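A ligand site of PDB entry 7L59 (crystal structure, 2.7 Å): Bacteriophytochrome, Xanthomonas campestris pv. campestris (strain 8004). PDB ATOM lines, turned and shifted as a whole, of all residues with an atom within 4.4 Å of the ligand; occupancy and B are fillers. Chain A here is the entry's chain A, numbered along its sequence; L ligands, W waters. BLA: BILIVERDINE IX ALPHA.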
ATOM      1  N   CYS A  19     -22.933 -14.844  36.865  1.00  0.00           N
ATOM      2  CA  CYS A  19     -23.180 -14.931  35.416  1.00  0.00           C
ATOM      3  C   CYS A  19     -22.295 -13.981  34.573  1.00  0.00           C
ATOM      4  O   CYS A  19     -22.260 -14.117  33.346  1.00  0.00           O
ATOM      5  CB  CYS A  19     -24.661 -14.717  35.120  1.00  0.00           C
ATOM      6  SG  CYS A  19     -25.304 -13.096  35.627  1.00  0.00           S
ATOM      7  N   ALA A  20     -21.569 -13.043  35.207  1.00  0.00           N
ATOM      8  CA  ALA A  20     -20.638 -12.129  34.542  1.00  0.00           C
ATOM      9  C   ALA A  20     -19.419 -12.904  34.017  1.00  0.00           C
ATOM     10  O   ALA A  20     -18.780 -12.481  33.054  1.00  0.00           O
ATOM     11  CB  ALA A  20     -20.185 -11.056  35.511  1.00  0.00           C
ATOM     12  N   ILE A  24     -20.345 -19.432  28.735  1.00  0.00           N
ATOM     13  CA  ILE A  24     -21.427 -19.517  27.765  1.00  0.00           C
ATOM     14  C   ILE A  24     -21.026 -20.274  26.480  1.00  0.00           C
ATOM     15  O   ILE A  24     -21.890 -20.462  25.624  1.00  0.00           O
ATOM     16  CB  ILE A  24     -21.971 -18.102  27.444  1.00  0.00           C
ATOM     17  CG1 ILE A  24     -20.875 -17.166  26.906  1.00  0.00           C
ATOM     18  CG2 ILE A  24     -22.725 -17.479  28.634  1.00  0.00           C
ATOM     19  CD1 ILE A  24     -21.357 -16.265  25.848  1.00  0.00           C
ATOM     20  N   TYR A 174     -26.372  -0.207  18.333  1.00  0.00           N
ATOM     21  CA  TYR A 174     -25.676   0.157  19.573  1.00  0.00           C
ATOM     22  C   TYR A 174     -24.293   0.660  19.310  1.00  0.00           C
ATOM     23  O   TYR A 174     -23.617   0.185  18.393  1.00  0.00           O
ATOM     24  CB  TYR A 174     -25.558  -0.997  20.587  1.00  0.00           C
ATOM     25  CG  TYR A 174     -26.786  -1.858  20.815  1.00  0.00           C
ATOM     26  CD1 TYR A 174     -28.025  -1.271  21.061  1.00  0.00           C
ATOM     27  CD2 TYR A 174     -26.691  -3.235  20.865  1.00  0.00           C
ATOM     28  CE1 TYR A 174     -29.153  -2.061  21.294  1.00  0.00           C
ATOM     29  CE2 TYR A 174     -27.803  -4.028  21.087  1.00  0.00           C
ATOM     30  CZ  TYR A 174     -29.047  -3.440  21.310  1.00  0.00           C
ATOM     31  OH  TYR A 174     -30.131  -4.235  21.585  1.00  0.00           O
ATOM     32  N   ILE A 184     -28.287   3.150  22.587  1.00  0.00           N
ATOM     33  CA  ILE A 184     -29.158   2.854  21.424  1.00  0.00           C
ATOM     34  C   ILE A 184     -29.240   4.134  20.571  1.00  0.00           C
ATOM     35  O   ILE A 184     -30.058   5.020  20.846  1.00  0.00           O
ATOM     36  CB  ILE A 184     -30.542   2.289  21.823  1.00  0.00           C
ATOM     37  CG1 ILE A 184     -30.394   1.092  22.784  1.00  0.00           C
ATOM     38  CG2 ILE A 184     -31.351   1.917  20.555  1.00  0.00           C
ATOM     39  CD1 ILE A 184     -31.682   0.497  23.310  1.00  0.00           C
ATOM     40  N   TYR A 196     -37.091   2.331  22.585  1.00  0.00           N
ATOM     41  CA  TYR A 196     -35.923   2.287  23.453  1.00  0.00           C
ATOM     42  C   TYR A 196     -34.808   3.201  22.925  1.00  0.00           C
ATOM     43  O   TYR A 196     -33.774   3.323  23.568  1.00  0.00           O
ATOM     44  CB  TYR A 196     -35.410   0.846  23.606  1.00  0.00           C
ATOM     45  CG  TYR A 196     -36.432  -0.148  24.132  1.00  0.00           C
ATOM     46  CD1 TYR A 196     -37.191   0.133  25.261  1.00  0.00           C
ATOM     47  CD2 TYR A 196     -36.567  -1.398  23.561  1.00  0.00           C
ATOM     48  CE1 TYR A 196     -38.115  -0.780  25.756  1.00  0.00           C
ATOM     49  CE2 TYR A 196     -37.484  -2.322  24.050  1.00  0.00           C
ATOM     50  CZ  TYR A 196     -38.264  -2.008  25.147  1.00  0.00           C
ATOM     51  OH  TYR A 196     -39.151  -2.935  25.626  1.00  0.00           O
ATOM     52  N   LEU A 199     -31.856   5.078  25.009  1.00  0.00           N
ATOM     53  CA  LEU A 199     -31.572   4.308  26.205  1.00  0.00           C
ATOM     54  C   LEU A 199     -30.142   3.881  26.168  1.00  0.00           C
ATOM     55  O   LEU A 199     -29.592   3.590  25.099  1.00  0.00           O
ATOM     56  CB  LEU A 199     -32.501   3.076  26.260  1.00  0.00           C
ATOM     57  CG  LEU A 199     -32.612   2.255  27.542  1.00  0.00           C
ATOM     58  CD1 LEU A 199     -33.996   1.652  27.685  1.00  0.00           C
ATOM     59  CD2 LEU A 199     -31.618   1.118  27.540  1.00  0.00           C
ATOM     60  N   TYR A 201     -27.413   1.275  28.576  1.00  0.00           N
ATOM     61  CA  TYR A 201     -27.402   0.153  29.497  1.00  0.00           C
ATOM     62  C   TYR A 201     -25.996  -0.034  30.004  1.00  0.00           C
ATOM     63  O   TYR A 201     -25.058   0.377  29.329  1.00  0.00           O
ATOM     64  CB  TYR A 201     -27.968  -1.133  28.850  1.00  0.00           C
ATOM     65  CG  TYR A 201     -27.326  -1.522  27.537  1.00  0.00           C
ATOM     66  CD1 TYR A 201     -26.146  -2.286  27.499  1.00  0.00           C
ATOM     67  CD2 TYR A 201     -27.916  -1.183  26.313  1.00  0.00           C
ATOM     68  CE1 TYR A 201     -25.565  -2.649  26.299  1.00  0.00           C
ATOM     69  CE2 TYR A 201     -27.352  -1.565  25.111  1.00  0.00           C
ATOM     70  CZ  TYR A 201     -26.171  -2.289  25.101  1.00  0.00           C
ATOM     71  OH  TYR A 201     -25.594  -2.632  23.893  1.00  0.00           O
ATOM     72  N   SER A 204     -22.099  -4.457  32.180  1.00  0.00           N
ATOM     73  CA  SER A 204     -22.409  -5.716  32.870  1.00  0.00           C
ATOM     74  C   SER A 204     -23.583  -6.477  32.242  1.00  0.00           C
ATOM     75  O   SER A 204     -23.736  -7.669  32.537  1.00  0.00           O
ATOM     76  CB  SER A 204     -22.722  -5.431  34.325  1.00  0.00           C
ATOM     77  OG  SER A 204     -23.914  -4.677  34.447  1.00  0.00           O
ATOM     78  N   ASP A 205     -24.391  -5.806  31.366  1.00  0.00           N
ATOM     79  CA  ASP A 205     -25.567  -6.375  30.679  1.00  0.00           C
ATOM     80  C   ASP A 205     -25.164  -7.314  29.568  1.00  0.00           C
ATOM     81  O   ASP A 205     -25.961  -8.145  29.188  1.00  0.00           O
ATOM     82  CB  ASP A 205     -26.470  -5.284  30.102  1.00  0.00           C
ATOM     83  CG  ASP A 205     -27.573  -4.775  31.021  1.00  0.00           C
ATOM     84  OD1 ASP A 205     -27.524  -5.079  32.248  1.00  0.00           O
ATOM     85  OD2 ASP A 205     -28.463  -4.078  30.526  1.00  0.00           O
ATOM     86  N   ILE A 206     -23.956  -7.133  29.006  1.00  0.00           N
ATOM     87  CA  ILE A 206     -23.386  -7.999  27.987  1.00  0.00           C
ATOM     88  C   ILE A 206     -22.015  -8.404  28.491  1.00  0.00           C
ATOM     89  O   ILE A 206     -21.096  -7.602  28.394  1.00  0.00           O
ATOM     90  CB  ILE A 206     -23.325  -7.393  26.536  1.00  0.00           C
ATOM     91  CG1 ILE A 206     -24.520  -6.445  26.222  1.00  0.00           C
ATOM     92  CG2 ILE A 206     -23.180  -8.518  25.493  1.00  0.00           C
ATOM     93  CD1 ILE A 206     -24.478  -5.738  24.882  1.00  0.00           C
ATOM     94  N   PRO A 207     -21.851  -9.590  29.111  1.00  0.00           N
ATOM     95  CA  PRO A 207     -20.523 -10.000  29.609  1.00  0.00           C
ATOM     96  C   PRO A 207     -19.442 -10.024  28.520  1.00  0.00           C
ATOM     97  O   PRO A 207     -19.716 -10.180  27.339  1.00  0.00           O
ATOM     98  CB  PRO A 207     -20.793 -11.423  30.127  1.00  0.00           C
ATOM     99  CG  PRO A 207     -22.230 -11.419  30.501  1.00  0.00           C
ATOM    100  CD  PRO A 207     -22.854 -10.635  29.391  1.00  0.00           C
ATOM    101  N   ALA A 210     -19.676 -12.810  26.072  1.00  0.00           N
ATOM    102  CA  ALA A 210     -20.802 -12.569  25.151  1.00  0.00           C
ATOM    103  C   ALA A 210     -20.320 -11.656  24.073  1.00  0.00           C
ATOM    104  O   ALA A 210     -20.371 -12.046  22.914  1.00  0.00           O
ATOM    105  CB  ALA A 210     -22.001 -11.968  25.887  1.00  0.00           C
ATOM    106  N   TYR A 214     -19.695 -12.439  19.981  1.00  0.00           N
ATOM    107  CA  TYR A 214     -20.390 -11.658  18.925  1.00  0.00           C
ATOM    108  C   TYR A 214     -19.374 -11.223  17.874  1.00  0.00           C
ATOM    109  O   TYR A 214     -19.645 -11.289  16.686  1.00  0.00           O
ATOM    110  CB  TYR A 214     -21.054 -10.418  19.517  1.00  0.00           C
ATOM    111  CG  TYR A 214     -22.347 -10.652  20.253  1.00  0.00           C
ATOM    112  CD1 TYR A 214     -23.334 -11.453  19.706  1.00  0.00           C
ATOM    113  CD2 TYR A 214     -22.607 -10.070  21.478  1.00  0.00           C
ATOM    114  CE1 TYR A 214     -24.523 -11.677  20.363  1.00  0.00           C
ATOM    115  CE2 TYR A 214     -23.796 -10.284  22.149  1.00  0.00           C
ATOM    116  CZ  TYR A 214     -24.755 -11.098  21.591  1.00  0.00           C
ATOM    117  OH  TYR A 214     -25.934 -11.323  22.228  1.00  0.00           O
ATOM    118  N   ARG A 220     -25.221 -13.535  15.213  1.00  0.00           N
ATOM    119  CA  ARG A 220     -25.721 -14.515  16.212  1.00  0.00           C
ATOM    120  C   ARG A 220     -27.250 -14.459  16.282  1.00  0.00           C
ATOM    121  O   ARG A 220     -27.768 -13.393  16.544  1.00  0.00           O
ATOM    122  CB  ARG A 220     -25.108 -14.184  17.577  1.00  0.00           C
ATOM    123  CG  ARG A 220     -25.007 -15.356  18.538  1.00  0.00           C
ATOM    124  CD  ARG A 220     -26.356 -15.764  19.076  1.00  0.00           C
ATOM    125  NE  ARG A 220     -26.320 -16.218  20.453  1.00  0.00           N
ATOM    126  CZ  ARG A 220     -26.282 -17.481  20.822  1.00  0.00           C
ATOM    127  NH1 ARG A 220     -26.258 -18.433  19.913  1.00  0.00           N
ATOM    128  NH2 ARG A 220     -26.253 -17.793  22.090  1.00  0.00           N
ATOM    129  N   ILE A 222     -31.163 -16.179  17.774  1.00  0.00           N
ATOM    130  CA  ILE A 222     -32.022 -16.851  18.746  1.00  0.00           C
ATOM    131  C   ILE A 222     -33.346 -16.973  18.009  1.00  0.00           C
ATOM    132  O   ILE A 222     -34.004 -15.950  17.819  1.00  0.00           O
ATOM    133  CB  ILE A 222     -32.130 -16.115  20.131  1.00  0.00           C
ATOM    134  CG1 ILE A 222     -30.733 -15.849  20.748  1.00  0.00           C
ATOM    135  CG2 ILE A 222     -33.076 -16.889  21.086  1.00  0.00           C
ATOM    136  CD1 ILE A 222     -30.711 -14.863  21.827  1.00  0.00           C
ATOM    137  N   SER A 253     -26.530 -22.642  22.423  1.00  0.00           N
ATOM    138  CA  SER A 253     -27.541 -22.283  23.398  1.00  0.00           C
ATOM    139  C   SER A 253     -27.297 -20.874  23.975  1.00  0.00           C
ATOM    140  O   SER A 253     -26.182 -20.344  23.920  1.00  0.00           O
ATOM    141  CB  SER A 253     -27.525 -23.297  24.540  1.00  0.00           C
ATOM    142  OG  SER A 253     -28.823 -23.809  24.750  1.00  0.00           O
ATOM    143  N   VAL A 254     -28.349 -20.257  24.522  1.00  0.00           N
ATOM    144  CA  VAL A 254     -28.245 -18.935  25.110  1.00  0.00           C
ATOM    145  C   VAL A 254     -28.432 -19.085  26.634  1.00  0.00           C
ATOM    146  O   VAL A 254     -29.076 -20.028  27.101  1.00  0.00           O
ATOM    147  CB  VAL A 254     -29.125 -17.835  24.414  1.00  0.00           C
ATOM    148  CG1 VAL A 254     -30.248 -18.419  23.585  1.00  0.00           C
ATOM    149  CG2 VAL A 254     -29.595 -16.717  25.352  1.00  0.00           C
ATOM    150  N   SER A 255     -27.710 -18.239  27.390  1.00  0.00           N
ATOM    151  CA  SER A 255     -27.737 -18.175  28.833  1.00  0.00           C
ATOM    152  C   SER A 255     -29.161 -17.972  29.329  1.00  0.00           C
ATOM    153  O   SER A 255     -29.858 -17.073  28.828  1.00  0.00           O
ATOM    154  CB  SER A 255     -26.841 -17.023  29.316  1.00  0.00           C
ATOM    155  OG  SER A 255     -27.194 -16.512  30.593  1.00  0.00           O
ATOM    156  N   VAL A 257     -30.154 -16.407  31.758  1.00  0.00           N
ATOM    157  CA  VAL A 257     -30.285 -15.019  32.217  1.00  0.00           C
ATOM    158  C   VAL A 257     -30.817 -14.174  31.053  1.00  0.00           C
ATOM    159  O   VAL A 257     -31.816 -13.450  31.215  1.00  0.00           O
ATOM    160  CB  VAL A 257     -28.973 -14.433  32.799  1.00  0.00           C
ATOM    161  CG1 VAL A 257     -29.262 -13.132  33.538  1.00  0.00           C
ATOM    162  CG2 VAL A 257     -28.275 -15.425  33.721  1.00  0.00           C
ATOM    163  N   HIS A 258     -30.161 -14.264  29.882  1.00  0.00           N
ATOM    164  CA  HIS A 258     -30.563 -13.502  28.700  1.00  0.00           C
ATOM    165  C   HIS A 258     -31.960 -13.920  28.249  1.00  0.00           C
ATOM    166  O   HIS A 258     -32.763 -13.051  27.942  1.00  0.00           O
ATOM    167  CB  HIS A 258     -29.544 -13.640  27.561  1.00  0.00           C
ATOM    168  CG  HIS A 258     -29.826 -12.709  26.415  1.00  0.00           C
ATOM    169  ND1 HIS A 258     -29.997 -11.346  26.612  1.00  0.00           N
ATOM    170  CD2 HIS A 258     -29.936 -12.971  25.098  1.00  0.00           C
ATOM    171  CE1 HIS A 258     -30.230 -10.842  25.417  1.00  0.00           C
ATOM    172  NE2 HIS A 258     -30.192 -11.775  24.473  1.00  0.00           N
ATOM    173  N   TYR A 261     -34.408 -12.174  30.322  1.00  0.00           N
ATOM    174  CA  TYR A 261     -34.437 -10.761  29.945  1.00  0.00           C
ATOM    175  C   TYR A 261     -35.407 -10.545  28.788  1.00  0.00           C
ATOM    176  O   TYR A 261     -36.309  -9.709  28.896  1.00  0.00           O
ATOM    177  CB  TYR A 261     -33.031 -10.259  29.549  1.00  0.00           C
ATOM    178  CG  TYR A 261     -32.906  -8.744  29.569  1.00  0.00           C
ATOM    179  CD1 TYR A 261     -33.512  -7.963  28.596  1.00  0.00           C
ATOM    180  CD2 TYR A 261     -32.147  -8.104  30.544  1.00  0.00           C
ATOM    181  CE1 TYR A 261     -33.432  -6.574  28.640  1.00  0.00           C
ATOM    182  CE2 TYR A 261     -32.054  -6.727  30.589  1.00  0.00           C
ATOM    183  CZ  TYR A 261     -32.715  -5.960  29.645  1.00  0.00           C
ATOM    184  OH  TYR A 261     -32.616  -4.603  29.684  1.00  0.00           O
ATOM    185  N   MET A 265     -39.552  -8.871  28.253  1.00  0.00           N
ATOM    186  CA  MET A 265     -39.759  -7.879  27.194  1.00  0.00           C
ATOM    187  C   MET A 265     -40.852  -8.284  26.217  1.00  0.00           C
ATOM    188  O   MET A 265     -41.375  -7.392  25.532  1.00  0.00           O
ATOM    189  CB  MET A 265     -38.449  -7.686  26.403  1.00  0.00           C
ATOM    190  CG  MET A 265     -37.535  -6.657  26.974  1.00  0.00           C
ATOM    191  SD  MET A 265     -35.977  -6.540  26.087  1.00  0.00           S
ATOM    192  CE  MET A 265     -36.466  -5.637  24.693  1.00  0.00           C
ATOM    193  N   THR A 270     -34.169 -13.110  18.150  1.00  0.00           N
ATOM    194  CA  THR A 270     -33.152 -12.057  17.986  1.00  0.00           C
ATOM    195  C   THR A 270     -32.105 -12.469  16.916  1.00  0.00           C
ATOM    196  O   THR A 270     -31.822 -13.663  16.711  1.00  0.00           O
ATOM    197  CB  THR A 270     -32.447 -11.635  19.326  1.00  0.00           C
ATOM    198  OG1 THR A 270     -31.435 -12.554  19.696  1.00  0.00           O
ATOM    199  CG2 THR A 270     -33.399 -11.434  20.495  1.00  0.00           C
ATOM    200  N   VAL A 272     -28.398 -10.702  16.068  1.00  0.00           N
ATOM    201  CA  VAL A 272     -27.395  -9.711  16.480  1.00  0.00           C
ATOM    202  C   VAL A 272     -26.204  -9.807  15.541  1.00  0.00           C
ATOM    203  O   VAL A 272     -25.712 -10.901  15.297  1.00  0.00           O
ATOM    204  CB  VAL A 272     -26.972  -9.884  17.975  1.00  0.00           C
ATOM    205  CG1 VAL A 272     -26.004  -8.779  18.410  1.00  0.00           C
ATOM    206  CG2 VAL A 272     -28.190  -9.886  18.876  1.00  0.00           C
ATOM    207  N   LEU A 284     -23.117  -3.020  17.951  1.00  0.00           N
ATOM    208  CA  LEU A 284     -23.859  -4.117  17.316  1.00  0.00           C
ATOM    209  C   LEU A 284     -25.153  -3.669  16.643  1.00  0.00           C
ATOM    210  O   LEU A 284     -25.710  -2.598  16.936  1.00  0.00           O
ATOM    211  CB  LEU A 284     -24.273  -5.226  18.326  1.00  0.00           C
ATOM    212  CG  LEU A 284     -23.405  -5.594  19.486  1.00  0.00           C
ATOM    213  CD1 LEU A 284     -24.264  -5.925  20.677  1.00  0.00           C
ATOM    214  CD2 LEU A 284     -22.436  -6.716  19.124  1.00  0.00           C
ATOM    215  N   SER A 286     -28.943  -5.070  16.574  1.00  0.00           N
ATOM    216  CA  SER A 286     -29.802  -6.002  17.284  1.00  0.00           C
ATOM    217  C   SER A 286     -31.218  -5.924  16.762  1.00  0.00           C
ATOM    218  O   SER A 286     -31.836  -4.876  16.720  1.00  0.00           O
ATOM    219  CB  SER A 286     -29.766  -5.753  18.784  1.00  0.00           C
ATOM    220  OG  SER A 286     -30.542  -6.724  19.476  1.00  0.00           O
ATOM    221  N   HIS A 288     -35.009  -7.509  17.057  1.00  0.00           N
ATOM    222  CA  HIS A 288     -35.905  -8.147  18.010  1.00  0.00           C
ATOM    223  C   HIS A 288     -37.234  -8.399  17.331  1.00  0.00           C
ATOM    224  O   HIS A 288     -37.789  -7.504  16.670  1.00  0.00           O
ATOM    225  CB  HIS A 288     -36.076  -7.313  19.302  1.00  0.00           C
ATOM    226  CG  HIS A 288     -34.893  -7.339  20.235  1.00  0.00           C
ATOM    227  ND1 HIS A 288     -34.933  -6.699  21.459  1.00  0.00           N
ATOM    228  CD2 HIS A 288     -33.684  -7.944  20.100  1.00  0.00           C
ATOM    229  CE1 HIS A 288     -33.752  -6.924  22.023  1.00  0.00           C
ATOM    230  NE2 HIS A 288     -32.962  -7.663  21.237  1.00  0.00           N
ATOM    231  N   LEU A 475     -35.242  -8.562  35.638  1.00  0.00           N
ATOM    232  CA  LEU A 475     -34.484  -7.899  34.553  1.00  0.00           C
ATOM    233  C   LEU A 475     -35.401  -7.106  33.619  1.00  0.00           C
ATOM    234  O   LEU A 475     -36.469  -7.618  33.259  1.00  0.00           O
ATOM    235  CB  LEU A 475     -33.708  -8.929  33.703  1.00  0.00           C
ATOM    236  CG  LEU A 475     -32.784  -9.932  34.411  1.00  0.00           C
ATOM    237  CD1 LEU A 475     -32.634 -11.209  33.605  1.00  0.00           C
ATOM    238  CD2 LEU A 475     -31.436  -9.328  34.727  1.00  0.00           C
ATOM    239  N   PRO A 477     -35.410  -3.377  30.449  1.00  0.00           N
ATOM    240  CA  PRO A 477     -34.832  -2.106  29.922  1.00  0.00           C
ATOM    241  C   PRO A 477     -34.860  -0.923  30.929  1.00  0.00           C
ATOM    242  O   PRO A 477     -33.921  -0.135  30.943  1.00  0.00           O
ATOM    243  CB  PRO A 477     -35.729  -1.796  28.716  1.00  0.00           C
ATOM    244  CG  PRO A 477     -36.217  -3.121  28.271  1.00  0.00           C
ATOM    245  CD  PRO A 477     -36.435  -3.900  29.525  1.00  0.00           C
ATOM    246  N   SER A 480     -32.158  -1.698  33.564  1.00  0.00           N
ATOM    247  CA  SER A 480     -30.856  -1.475  32.921  1.00  0.00           C
ATOM    248  C   SER A 480     -30.540   0.011  32.766  1.00  0.00           C
ATOM    249  O   SER A 480     -29.431   0.409  33.095  1.00  0.00           O
ATOM    250  CB  SER A 480     -30.811  -2.155  31.563  1.00  0.00           C
ATOM    251  OG  SER A 480     -30.786  -3.556  31.754  1.00  0.00           O
HETATM  252  CHA BLA L   1     -26.747 -10.194  25.596  1.00  0.00           C
HETATM  253  NA  BLA L   1     -28.043  -8.360  26.852  1.00  0.00           N
HETATM  254  C1A BLA L   1     -27.414  -8.830  25.745  1.00  0.00           C
HETATM  255  C2A BLA L   1     -27.514  -7.879  24.763  1.00  0.00           C
HETATM  256  C3A BLA L   1     -28.197  -6.817  25.254  1.00  0.00           C
HETATM  257  C4A BLA L   1     -28.540  -7.132  26.567  1.00  0.00           C
HETATM  258  CMA BLA L   1     -28.533  -5.532  24.483  1.00  0.00           C
HETATM  259  CAA BLA L   1     -26.979  -8.026  23.314  1.00  0.00           C
HETATM  260  CBA BLA L   1     -27.972  -8.975  22.518  1.00  0.00           C
HETATM  261  CGA BLA L   1     -29.312  -8.343  22.073  1.00  0.00           C
HETATM  262  O1A BLA L   1     -29.401  -7.116  21.854  1.00  0.00           O
HETATM  263  O2A BLA L   1     -30.328  -9.072  21.871  1.00  0.00           O
HETATM  264  CHB BLA L   1     -29.328  -6.304  27.574  1.00  0.00           C
HETATM  265  NB  BLA L   1     -30.166  -3.999  28.036  1.00  0.00           N
HETATM  266  C1B BLA L   1     -30.154  -5.313  27.270  1.00  0.00           C
HETATM  267  C2B BLA L   1     -31.274  -5.192  26.258  1.00  0.00           C
HETATM  268  C3B BLA L   1     -31.890  -3.913  26.336  1.00  0.00           C
HETATM  269  C4B BLA L   1     -31.253  -3.120  27.430  1.00  0.00           C
HETATM  270  CMB BLA L   1     -31.727  -6.255  25.239  1.00  0.00           C
HETATM  271  OB  BLA L   1     -31.526  -2.039  27.808  1.00  0.00           O
HETATM  272  CAB BLA L   1     -33.064  -3.456  25.457  1.00  0.00           C
HETATM  273  CBB BLA L   1     -33.640  -2.282  25.583  1.00  0.00           C
HETATM  274  NC  BLA L   1     -27.984 -10.271  30.871  1.00  0.00           N
HETATM  275  C1C BLA L   1     -28.286  -9.403  32.089  1.00  0.00           C
HETATM  276  C2C BLA L   1     -27.185  -9.692  33.064  1.00  0.00           C
HETATM  277  C3C BLA L   1     -26.262 -10.648  32.524  1.00  0.00           C
HETATM  278  C4C BLA L   1     -26.689 -11.048  31.161  1.00  0.00           C
HETATM  279  CMC BLA L   1     -27.055  -8.990  34.415  1.00  0.00           C
HETATM  280  OC  BLA L   1     -29.187  -8.648  32.240  1.00  0.00           O
HETATM  281  CAC BLA L   1     -25.004 -11.152  33.207  1.00  0.00           C
HETATM  282  CBC BLA L   1     -25.089 -11.924  34.270  1.00  0.00           C
HETATM  283  CHD BLA L   1     -26.103 -11.938  30.393  1.00  0.00           C
HETATM  284  ND  BLA L   1     -26.595 -10.657  28.084  1.00  0.00           N
HETATM  285  C1D BLA L   1     -26.112 -11.817  28.866  1.00  0.00           C
HETATM  286  C2D BLA L   1     -25.609 -12.838  27.974  1.00  0.00           C
HETATM  287  C3D BLA L   1     -25.769 -12.321  26.547  1.00  0.00           C
HETATM  288  C4D BLA L   1     -26.417 -10.948  26.619  1.00  0.00           C
HETATM  289  CMD BLA L   1     -25.009 -14.188  28.359  1.00  0.00           C
HETATM  290  CAD BLA L   1     -25.417 -13.022  25.242  1.00  0.00           C
HETATM  291  CBD BLA L   1     -26.630 -13.992  24.981  1.00  0.00           C
HETATM  292  CGD BLA L   1     -26.351 -14.868  23.768  1.00  0.00           C
HETATM  293  O1D BLA L   1     -25.900 -16.011  23.968  1.00  0.00           O
HETATM  294  O2D BLA L   1     -26.583 -14.465  22.588  1.00  0.00           O
HETATM  295  O   HOH W   1     -28.247 -12.566  20.982  1.00  0.00           O
HETATM  296  O   HOH W   2     -29.576  -9.733  28.778  1.00  0.00           O
HETATM  297  O   HOH W   3     -23.105 -16.029  22.874  1.00  0.00           O
HETATM  298  O   HOH W   4     -25.399 -17.292  26.207  1.00  0.00           O
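The backbone NH of Arg 220 sits at hydrogen-bond distance from the backbone carbonyl oxygen of Val 272, 2.7 Å away. The guanidinium group (NH2) of Arg 220 is in hydrogen-bond range of the backbone carbonyl oxygen (O) of Ser 253 (3.1 Å). OG of Ser 286 lies within hydrogen-bond range of NE2 of His 288, at 3.1 Å. The side-chain carboxylate (OD2) of Asp 205 is in hydrogen-bond range of the side-chain hydroxyl (OG) of Ser 480 (2.7 Å). The backbone NH of Tyr 174 is in hydrogen-bond range of the backbone carbonyl oxygen of Leu 284, 2.8 Å away. OH of Tyr 261 sits at hydrogen-bond distance from OG of Ser 480, at 3.0 Å. The backbone carbonyl oxygen (O) of Leu 199 lies within hydrogen-bond range of the backbone NH (N) of Ile 184. The side-chain hydroxyl (OG) of Ser 255 lies close to the backbone NH (N) of Val 257 (3.2 Å).
Ala 20 touches the ligand (N to CBC, 3.8 Å). Tyr 196 touches the ligand (CD2 to CBB, 3.7 Å). Leu 199 touches the ligand. Tyr 201 touches the ligand (CB to NB, 3.7 Å). O of Ser 204 touches CAC of the ligand, 3.8 Å away. CG1 of Ile 206 touches C2A of the ligand, 3.6 Å away. CD of Pro 207 touches C1D of the ligand (3.5 Å). Ala 210 touches the ligand. CB of Val 254 touches O1D of the ligand, at 3.7 Å. Ser 255 touches the ligand. His 258 touches the ligand (CD2 to CBD, 3.5 Å). Val 272 touches the ligand (CG2 to CGA, 3.7 Å). Leu 475 touches the ligand. Pro 477 touches the ligand. OG of Ser 480 touches NB of the ligand, at 3.8 Å. Hydrophobic or aromatic side chains that line the ligand: Tyr 174, Tyr 196, Leu 199, Tyr 201, Ile 206, Pro 207, Ala 210, Tyr 214, Val 254, His 258, Tyr 261, Val 272, His 288, Leu 475 and Pro 477. Of the 31 residues printed, 23 come within 4 Å of the ligand. The nearest printed residue that does not touch the ligand is Ile 24 (4.02 Å).
A carbon (CBC) of the ligand is bonded to the side-chain sulfur (SG) of Cys 19 (1.8 Å). O1D of the ligand lies within salt-bridge range of NH2 of Arg 220, at 2.6 Å. O1A of the ligand is in hydrogen-bond range of OG of Ser 286, at 2.7 Å. O of Asp 205 is in hydrogen-bond range of NA of the ligand, 3.1 Å away. The side-chain carboxylate (OD2) of Asp 205 sits at hydrogen-bond distance from a nitrogen (NB) of the ligand (3.0 Å). The side-chain hydroxyl (OH) of Tyr 174 is in hydrogen-bond range of an oxygen (O1A) of the ligand (3.0 Å). OH of Tyr 261 lies within hydrogen-bond range of NB of the ligand (3.0 Å). A ring nitrogen (NE2) of His 288 lies within hydrogen-bond range of an oxygen (O2A) of the ligand (3.1 Å). OH of Tyr 214 sits close to O2D of the ligand, 3.2 Å away.
Water W4 bridges O1D of the ligand (2.6 Å) and N of Ser 255 (2.8 Å). Water W2 bridges a nitrogen (NC) of the ligand (2.7 Å) and a ring nitrogen (ND1) of His 258 (2.7 Å). Water W1 lies within hydrogen-bond range of OH of Tyr 214 (2.9 Å), O2D of the ligand (3.0 Å) and OG1 of Thr 270 (3.4 Å).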
